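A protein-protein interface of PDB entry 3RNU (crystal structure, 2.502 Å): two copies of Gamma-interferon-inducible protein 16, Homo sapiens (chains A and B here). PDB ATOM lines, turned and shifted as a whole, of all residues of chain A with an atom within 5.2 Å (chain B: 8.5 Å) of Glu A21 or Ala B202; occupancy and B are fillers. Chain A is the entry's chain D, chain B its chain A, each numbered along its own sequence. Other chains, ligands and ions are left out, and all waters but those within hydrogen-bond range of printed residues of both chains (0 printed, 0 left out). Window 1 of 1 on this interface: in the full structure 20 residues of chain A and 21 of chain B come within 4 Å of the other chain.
Hydrophobic or aromatic side chains of chain B that line the printed part of chain A: Ala B202 and Ala B203.
Among the printed residues, 11 pairs touch across the chains.
No position is printed for both chains.
Of the 11 pairs that touch across the chains among the printed residues, none has its exchanged pair printed and touching as well.
Of the printed residues of chain B, Ala A19 touches Ala B202 (3.3 Å) and Ala B203 (2.6 Å).
Thr A20 touches just one residue of chain B: Ala B202.
Of chain B, only Asn B160, Asn B200 and Ala B202 come within 4 Å of Glu A21.
Phe A23 touches none of the printed residues of chain B.
Printed residues of chain B within 4 Å of Lys A55: Lys B199 (3.5 Å), Asn B200 (3.5 Å) and Ala B201 (3.2 Å).
Printed residues of chain A within 4 Å of Lys B199: Lys A55.
Of the printed residues of chain A, Ala B201 touches Lys A55 (3.2 Å).
Of chain A, only Ala A19 (3.3 Å), Thr A20 (3.8 Å) and Glu A21 (3.4 Å) come within 4 Å of Ala B202.
The nearest printed residue of chain A that does not touch Asn B160 is Phe A23 (4.2 Å).
Ala A19 touches Ala B202 (O to CA, 3.3 Å).
Thr A20 touches Ala B202.
Glu A21 touches Asn B160 (CG to ND2, 3.96 Å).
Glu A21 touches Asn B200.
Glu A21 touches Ala B202.
Asn B200 touches Ser A22 (O to N, 3.98 Å).
Lys A55 touches Lys B199.
Asn B200 touches Lys A55 (O to CE, 3.5 Å).
The backbone NH (N) of Thr A20 sits at hydrogen-bond distance from the backbone carbonyl oxygen (O) of His A35, 2.9 Å away.
O of Thr A20 lies close to NZ of Lys A55 (3.1 Å).
A ring nitrogen (NE2) of His A191 sits at hydrogen-bond distance from the side-chain carboxylate of Glu A21 (3.1 Å).
O of Ser A22 sits at hydrogen-bond distance from ND2 of Asn B160 (3.2 Å).
The side-chain amino group of Lys A55 is in hydrogen-bond range of the backbone carbonyl oxygen of Ala B201.
The backbone carbonyl oxygen of Ala A19 is in hydrogen-bond range of the backbone NH of Ala B203 (2.6 Å).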
ATOM      1  N   ALA A  19       6.665   6.744  18.018  1.00  0.00           N
ATOM      2  CA  ALA A  19       5.342   6.158  18.207  1.00  0.00           C
ATOM      3  C   ALA A  19       4.308   7.266  18.297  1.00  0.00           C
ATOM      4  O   ALA A  19       4.518   8.259  18.993  1.00  0.00           O
ATOM      5  CB  ALA A  19       5.309   5.307  19.462  1.00  0.00           C
ATOM      6  N   THR A  20       3.195   7.112  17.594  1.00  0.00           N
ATOM      7  CA  THR A  20       2.135   8.088  17.714  1.00  0.00           C
ATOM      8  C   THR A  20       1.439   7.861  19.044  1.00  0.00           C
ATOM      9  O   THR A  20       1.792   6.957  19.785  1.00  0.00           O
ATOM     10  CB  THR A  20       1.130   7.949  16.564  1.00  0.00           C
ATOM     11  OG1 THR A  20       0.357   6.752  16.741  1.00  0.00           O
ATOM     12  CG2 THR A  20       1.874   7.890  15.234  1.00  0.00           C
ATOM     13  N   GLU A  21       0.463   8.700  19.354  1.00  0.00           N
ATOM     14  CA  GLU A  21      -0.386   8.479  20.511  1.00  0.00           C
ATOM     15  C   GLU A  21      -1.336   7.333  20.199  1.00  0.00           C
ATOM     16  O   GLU A  21      -1.426   6.893  19.052  1.00  0.00           O
ATOM     17  CB  GLU A  21      -1.153   9.743  20.907  1.00  0.00           C
ATOM     18  CG  GLU A  21      -2.262  10.149  19.947  1.00  0.00           C
ATOM     19  CD  GLU A  21      -1.742  10.765  18.663  1.00  0.00           C
ATOM     20  OE1 GLU A  21      -0.512  10.976  18.551  1.00  0.00           O
ATOM     21  OE2 GLU A  21      -2.569  11.038  17.765  1.00  0.00           O
ATOM     22  N   SER A  22      -1.974   6.793  21.230  1.00  0.00           N
ATOM     23  CA  SER A  22      -3.034   5.811  21.030  1.00  0.00           C
ATOM     24  C   SER A  22      -4.366   6.488  20.690  1.00  0.00           C
ATOM     25  O   SER A  22      -4.884   7.300  21.459  1.00  0.00           O
ATOM     26  CB  SER A  22      -3.182   4.918  22.264  1.00  0.00           C
ATOM     27  OG  SER A  22      -2.909   5.634  23.456  1.00  0.00           O
ATOM     28  N   PHE A  23      -4.919   6.135  19.536  1.00  0.00           N
ATOM     29  CA  PHE A  23      -6.115   6.784  19.018  1.00  0.00           C
ATOM     30  C   PHE A  23      -7.198   5.767  18.640  1.00  0.00           C
ATOM     31  O   PHE A  23      -6.931   4.570  18.566  1.00  0.00           O
ATOM     32  CB  PHE A  23      -5.769   7.654  17.801  1.00  0.00           C
ATOM     33  CG  PHE A  23      -5.392   6.865  16.574  1.00  0.00           C
ATOM     34  CD1 PHE A  23      -6.353   6.502  15.644  1.00  0.00           C
ATOM     35  CD2 PHE A  23      -4.080   6.482  16.354  1.00  0.00           C
ATOM     36  CE1 PHE A  23      -6.013   5.774  14.520  1.00  0.00           C
ATOM     37  CE2 PHE A  23      -3.738   5.753  15.228  1.00  0.00           C
ATOM     38  CZ  PHE A  23      -4.707   5.400  14.313  1.00  0.00           C
ATOM     39  N   MET A  33      -5.702   1.929  18.365  1.00  0.00           N
ATOM     40  CA  MET A  33      -4.396   1.498  17.864  1.00  0.00           C
ATOM     41  C   MET A  33      -3.410   2.646  17.977  1.00  0.00           C
ATOM     42  O   MET A  33      -3.812   3.788  18.168  1.00  0.00           O
ATOM     43  CB  MET A  33      -4.484   1.107  16.388  1.00  0.00           C
ATOM     44  CG  MET A  33      -4.414   2.301  15.455  1.00  0.00           C
ATOM     45  SD  MET A  33      -4.489   1.870  13.715  1.00  0.00           S
ATOM     46  CE  MET A  33      -2.929   1.018  13.525  1.00  0.00           C
ATOM     47  N   PHE A  34      -2.120   2.354  17.862  1.00  0.00           N
ATOM     48  CA  PHE A  34      -1.144   3.405  17.575  1.00  0.00           C
ATOM     49  C   PHE A  34      -0.177   2.912  16.510  1.00  0.00           C
ATOM     50  O   PHE A  34      -0.030   1.715  16.319  1.00  0.00           O
ATOM     51  CB  PHE A  34      -0.418   3.883  18.838  1.00  0.00           C
ATOM     52  CG  PHE A  34       0.416   2.822  19.516  1.00  0.00           C
ATOM     53  CD1 PHE A  34      -0.124   2.045  20.532  1.00  0.00           C
ATOM     54  CD2 PHE A  34       1.741   2.622  19.154  1.00  0.00           C
ATOM     55  CE1 PHE A  34       0.627   1.092  21.157  1.00  0.00           C
ATOM     56  CE2 PHE A  34       2.502   1.666  19.774  1.00  0.00           C
ATOM     57  CZ  PHE A  34       1.946   0.898  20.780  1.00  0.00           C
ATOM     58  N   HIS A  35       0.446   3.833  15.791  1.00  0.00           N
ATOM     59  CA  HIS A  35       1.405   3.475  14.754  1.00  0.00           C
ATOM     60  C   HIS A  35       2.802   3.692  15.295  1.00  0.00           C
ATOM     61  O   HIS A  35       3.035   4.599  16.091  1.00  0.00           O
ATOM     62  CB  HIS A  35       1.229   4.351  13.510  1.00  0.00           C
ATOM     63  CG  HIS A  35      -0.100   4.209  12.836  1.00  0.00           C
ATOM     64  ND1 HIS A  35      -0.366   3.216  11.920  1.00  0.00           N
ATOM     65  CD2 HIS A  35      -1.226   4.957  12.920  1.00  0.00           C
ATOM     66  CE1 HIS A  35      -1.605   3.348  11.481  1.00  0.00           C
ATOM     67  NE2 HIS A  35      -2.148   4.398  12.071  1.00  0.00           N
ATOM     68  N   LYS A  55       2.145   0.637  24.541  1.00  0.00           N
ATOM     69  CA  LYS A  55       2.615   1.999  24.327  1.00  0.00           C
ATOM     70  C   LYS A  55       3.950   2.233  25.032  1.00  0.00           C
ATOM     71  O   LYS A  55       4.914   2.707  24.426  1.00  0.00           O
ATOM     72  CB  LYS A  55       1.564   3.005  24.801  1.00  0.00           C
ATOM     73  CG  LYS A  55       1.878   4.455  24.464  1.00  0.00           C
ATOM     74  CD  LYS A  55       1.463   4.817  23.050  1.00  0.00           C
ATOM     75  CE  LYS A  55       1.686   6.301  22.761  1.00  0.00           C
ATOM     76  NZ  LYS A  55       3.125   6.638  22.578  1.00  0.00           N
ATOM     77  N   HIS A 191      -4.043   8.050  10.039  1.00  0.00           N
ATOM     78  CA  HIS A 191      -3.822   8.957  11.163  1.00  0.00           C
ATOM     79  C   HIS A 191      -3.225  10.264  10.650  1.00  0.00           C
ATOM     80  O   HIS A 191      -2.441  10.271   9.695  1.00  0.00           O
ATOM     81  CB  HIS A 191      -2.869   8.313  12.176  1.00  0.00           C
ATOM     82  CG  HIS A 191      -2.238   9.278  13.133  1.00  0.00           C
ATOM     83  ND1 HIS A 191      -1.168  10.078  12.791  1.00  0.00           N
ATOM     84  CD2 HIS A 191      -2.511   9.549  14.433  1.00  0.00           C
ATOM     85  CE1 HIS A 191      -0.821  10.814  13.833  1.00  0.00           C
ATOM     86  NE2 HIS A 191      -1.620  10.512  14.841  1.00  0.00           N
ATOM     87  N   ASN B 160     -10.053  12.818  21.012  1.00  0.00           N
ATOM     88  CA  ASN B 160      -9.310  11.780  21.683  1.00  0.00           C
ATOM     89  C   ASN B 160      -8.883  12.282  23.042  1.00  0.00           C
ATOM     90  O   ASN B 160      -7.916  13.029  23.181  1.00  0.00           O
ATOM     91  CB  ASN B 160      -8.077  11.401  20.869  1.00  0.00           C
ATOM     92  CG  ASN B 160      -7.283  10.287  21.509  1.00  0.00           C
ATOM     93  OD1 ASN B 160      -7.839   9.413  22.170  1.00  0.00           O
ATOM     94  ND2 ASN B 160      -5.973  10.316  21.319  1.00  0.00           N
ATOM     95  N   GLU B 162      -8.532  10.387  26.903  1.00  0.00           N
ATOM     96  CA  GLU B 162      -8.640   9.122  27.600  1.00  0.00           C
ATOM     97  C   GLU B 162      -8.474   9.337  29.089  1.00  0.00           C
ATOM     98  O   GLU B 162      -7.999  10.384  29.528  1.00  0.00           O
ATOM     99  CB  GLU B 162      -7.609   8.124  27.073  1.00  0.00           C
ATOM    100  CG  GLU B 162      -7.872   7.681  25.643  1.00  0.00           C
ATOM    101  CD  GLU B 162      -9.265   7.100  25.458  1.00  0.00           C
ATOM    102  OE1 GLU B 162      -9.796   6.496  26.416  1.00  0.00           O
ATOM    103  OE2 GLU B 162      -9.831   7.248  24.354  1.00  0.00           O
ATOM    104  N   ASP B 165      -6.121  11.925  30.981  1.00  0.00           N
ATOM    105  CA  ASP B 165      -5.814  13.176  30.294  1.00  0.00           C
ATOM    106  C   ASP B 165      -6.462  14.369  30.991  1.00  0.00           C
ATOM    107  O   ASP B 165      -7.215  14.212  31.954  1.00  0.00           O
ATOM    108  CB  ASP B 165      -6.250  13.121  28.826  1.00  0.00           C
ATOM    109  CG  ASP B 165      -5.362  12.224  27.984  1.00  0.00           C
ATOM    110  OD1 ASP B 165      -4.158  12.117  28.293  1.00  0.00           O
ATOM    111  OD2 ASP B 165      -5.869  11.621  27.014  1.00  0.00           O
ATOM    112  N   LYS B 196      -2.706  15.689  26.951  1.00  0.00           N
ATOM    113  CA  LYS B 196      -2.304  14.321  27.251  1.00  0.00           C
ATOM    114  C   LYS B 196      -1.058  14.257  28.133  1.00  0.00           C
ATOM    115  O   LYS B 196      -0.154  15.084  28.002  1.00  0.00           O
ATOM    116  CB  LYS B 196      -2.074  13.532  25.960  1.00  0.00           C
ATOM    117  CG  LYS B 196      -3.322  12.867  25.405  1.00  0.00           C
ATOM    118  CD  LYS B 196      -3.053  12.225  24.055  1.00  0.00           C
ATOM    119  CE  LYS B 196      -4.211  11.342  23.619  1.00  0.00           C
ATOM    120  NZ  LYS B 196      -4.274  10.058  24.376  1.00  0.00           N
ATOM    121  N   THR B 197      -1.026  13.286  29.042  1.00  0.00           N
ATOM    122  CA  THR B 197       0.192  12.967  29.779  1.00  0.00           C
ATOM    123  C   THR B 197       1.204  12.425  28.779  1.00  0.00           C
ATOM    124  O   THR B 197       0.817  11.849  27.763  1.00  0.00           O
ATOM    125  CB  THR B 197      -0.066  11.917  30.865  1.00  0.00           C
ATOM    126  OG1 THR B 197       1.181  11.480  31.420  1.00  0.00           O
ATOM    127  CG2 THR B 197      -0.791  10.724  30.278  1.00  0.00           C
ATOM    128  N   ARG B 198       2.486  12.636  29.060  1.00  0.00           N
ATOM    129  CA  ARG B 198       3.555  12.310  28.123  1.00  0.00           C
ATOM    130  C   ARG B 198       3.597  10.842  27.709  1.00  0.00           C
ATOM    131  O   ARG B 198       3.956  10.523  26.575  1.00  0.00           O
ATOM    132  CB  ARG B 198       4.911  12.726  28.699  1.00  0.00           C
ATOM    133  CG  ARG B 198       5.989  12.950  27.651  1.00  0.00           C
ATOM    134  CD  ARG B 198       7.105  13.831  28.186  1.00  0.00           C
ATOM    135  NE  ARG B 198       8.075  13.072  28.969  1.00  0.00           N
ATOM    136  CZ  ARG B 198       8.216  13.175  30.287  1.00  0.00           C
ATOM    137  NH1 ARG B 198       7.450  14.010  30.974  1.00  0.00           N
ATOM    138  NH2 ARG B 198       9.126  12.445  30.918  1.00  0.00           N
ATOM    139  N   LYS B 199       3.241   9.948  28.625  1.00  0.00           N
ATOM    140  CA  LYS B 199       3.351   8.519  28.357  1.00  0.00           C
ATOM    141  C   LYS B 199       2.308   8.081  27.330  1.00  0.00           C
ATOM    142  O   LYS B 199       2.524   7.125  26.585  1.00  0.00           O
ATOM    143  CB  LYS B 199       3.261   7.691  29.643  1.00  0.00           C
ATOM    144  CG  LYS B 199       1.903   7.676  30.320  1.00  0.00           C
ATOM    145  CD  LYS B 199       1.911   6.677  31.469  1.00  0.00           C
ATOM    146  CE  LYS B 199       0.522   6.446  32.038  1.00  0.00           C
ATOM    147  NZ  LYS B 199       0.532   5.389  33.089  1.00  0.00           N
ATOM    148  N   ASN B 200       1.175   8.781  27.309  1.00  0.00           N
ATOM    149  CA  ASN B 200       0.145   8.586  26.290  1.00  0.00           C
ATOM    150  C   ASN B 200       0.389   9.379  25.002  1.00  0.00           C
ATOM    151  O   ASN B 200      -0.169   9.060  23.951  1.00  0.00           O
ATOM    152  CB  ASN B 200      -1.234   8.947  26.848  1.00  0.00           C
ATOM    153  CG  ASN B 200      -1.582   8.167  28.099  1.00  0.00           C
ATOM    154  OD1 ASN B 200      -0.966   7.144  28.400  1.00  0.00           O
ATOM    155  ND2 ASN B 200      -2.583   8.644  28.832  1.00  0.00           N
ATOM    156  N   ALA B 201       1.213  10.420  25.101  1.00  0.00           N
ATOM    157  CA  ALA B 201       1.473  11.327  23.984  1.00  0.00           C
ATOM    158  C   ALA B 201       2.394  10.726  22.922  1.00  0.00           C
ATOM    159  O   ALA B 201       3.139   9.787  23.193  1.00  0.00           O
ATOM    160  CB  ALA B 201       2.040  12.649  24.499  1.00  0.00           C
ATOM    161  N   ALA B 202       2.343  11.279  21.714  1.00  0.00           N
ATOM    162  CA  ALA B 202       3.173  10.799  20.611  1.00  0.00           C
ATOM    163  C   ALA B 202       4.657  11.009  20.910  1.00  0.00           C
ATOM    164  O   ALA B 202       5.012  11.859  21.724  1.00  0.00           O
ATOM    165  CB  ALA B 202       2.780  11.490  19.310  1.00  0.00           C
ATOM    166  N   ALA B 203       5.523  10.234  20.265  1.00  0.00           N
ATOM    167  CA  ALA B 203       6.950  10.293  20.563  1.00  0.00           C
ATOM    168  C   ALA B 203       7.838  10.087  19.335  1.00  0.00           C
ATOM    169  O   ALA B 203       7.389   9.567  18.313  1.00  0.00           O
ATOM    170  CB  ALA B 203       7.302   9.286  21.653  1.00  0.00           C
ATOM    171  N   SER B 204       9.099  10.505  19.454  1.00  0.00           N
ATOM    172  CA  SER B 204      10.101  10.345  18.399  1.00  0.00           C
ATOM    173  C   SER B 204      11.471  10.810  18.880  1.00  0.00           C
ATOM    174  O   SER B 204      11.826  10.622  20.045  1.00  0.00           O
ATOM    175  CB  SER B 204       9.708  11.118  17.139  1.00  0.00           C
ATOM    176  OG  SER B 204       9.686  12.514  17.372  1.00  0.00           O
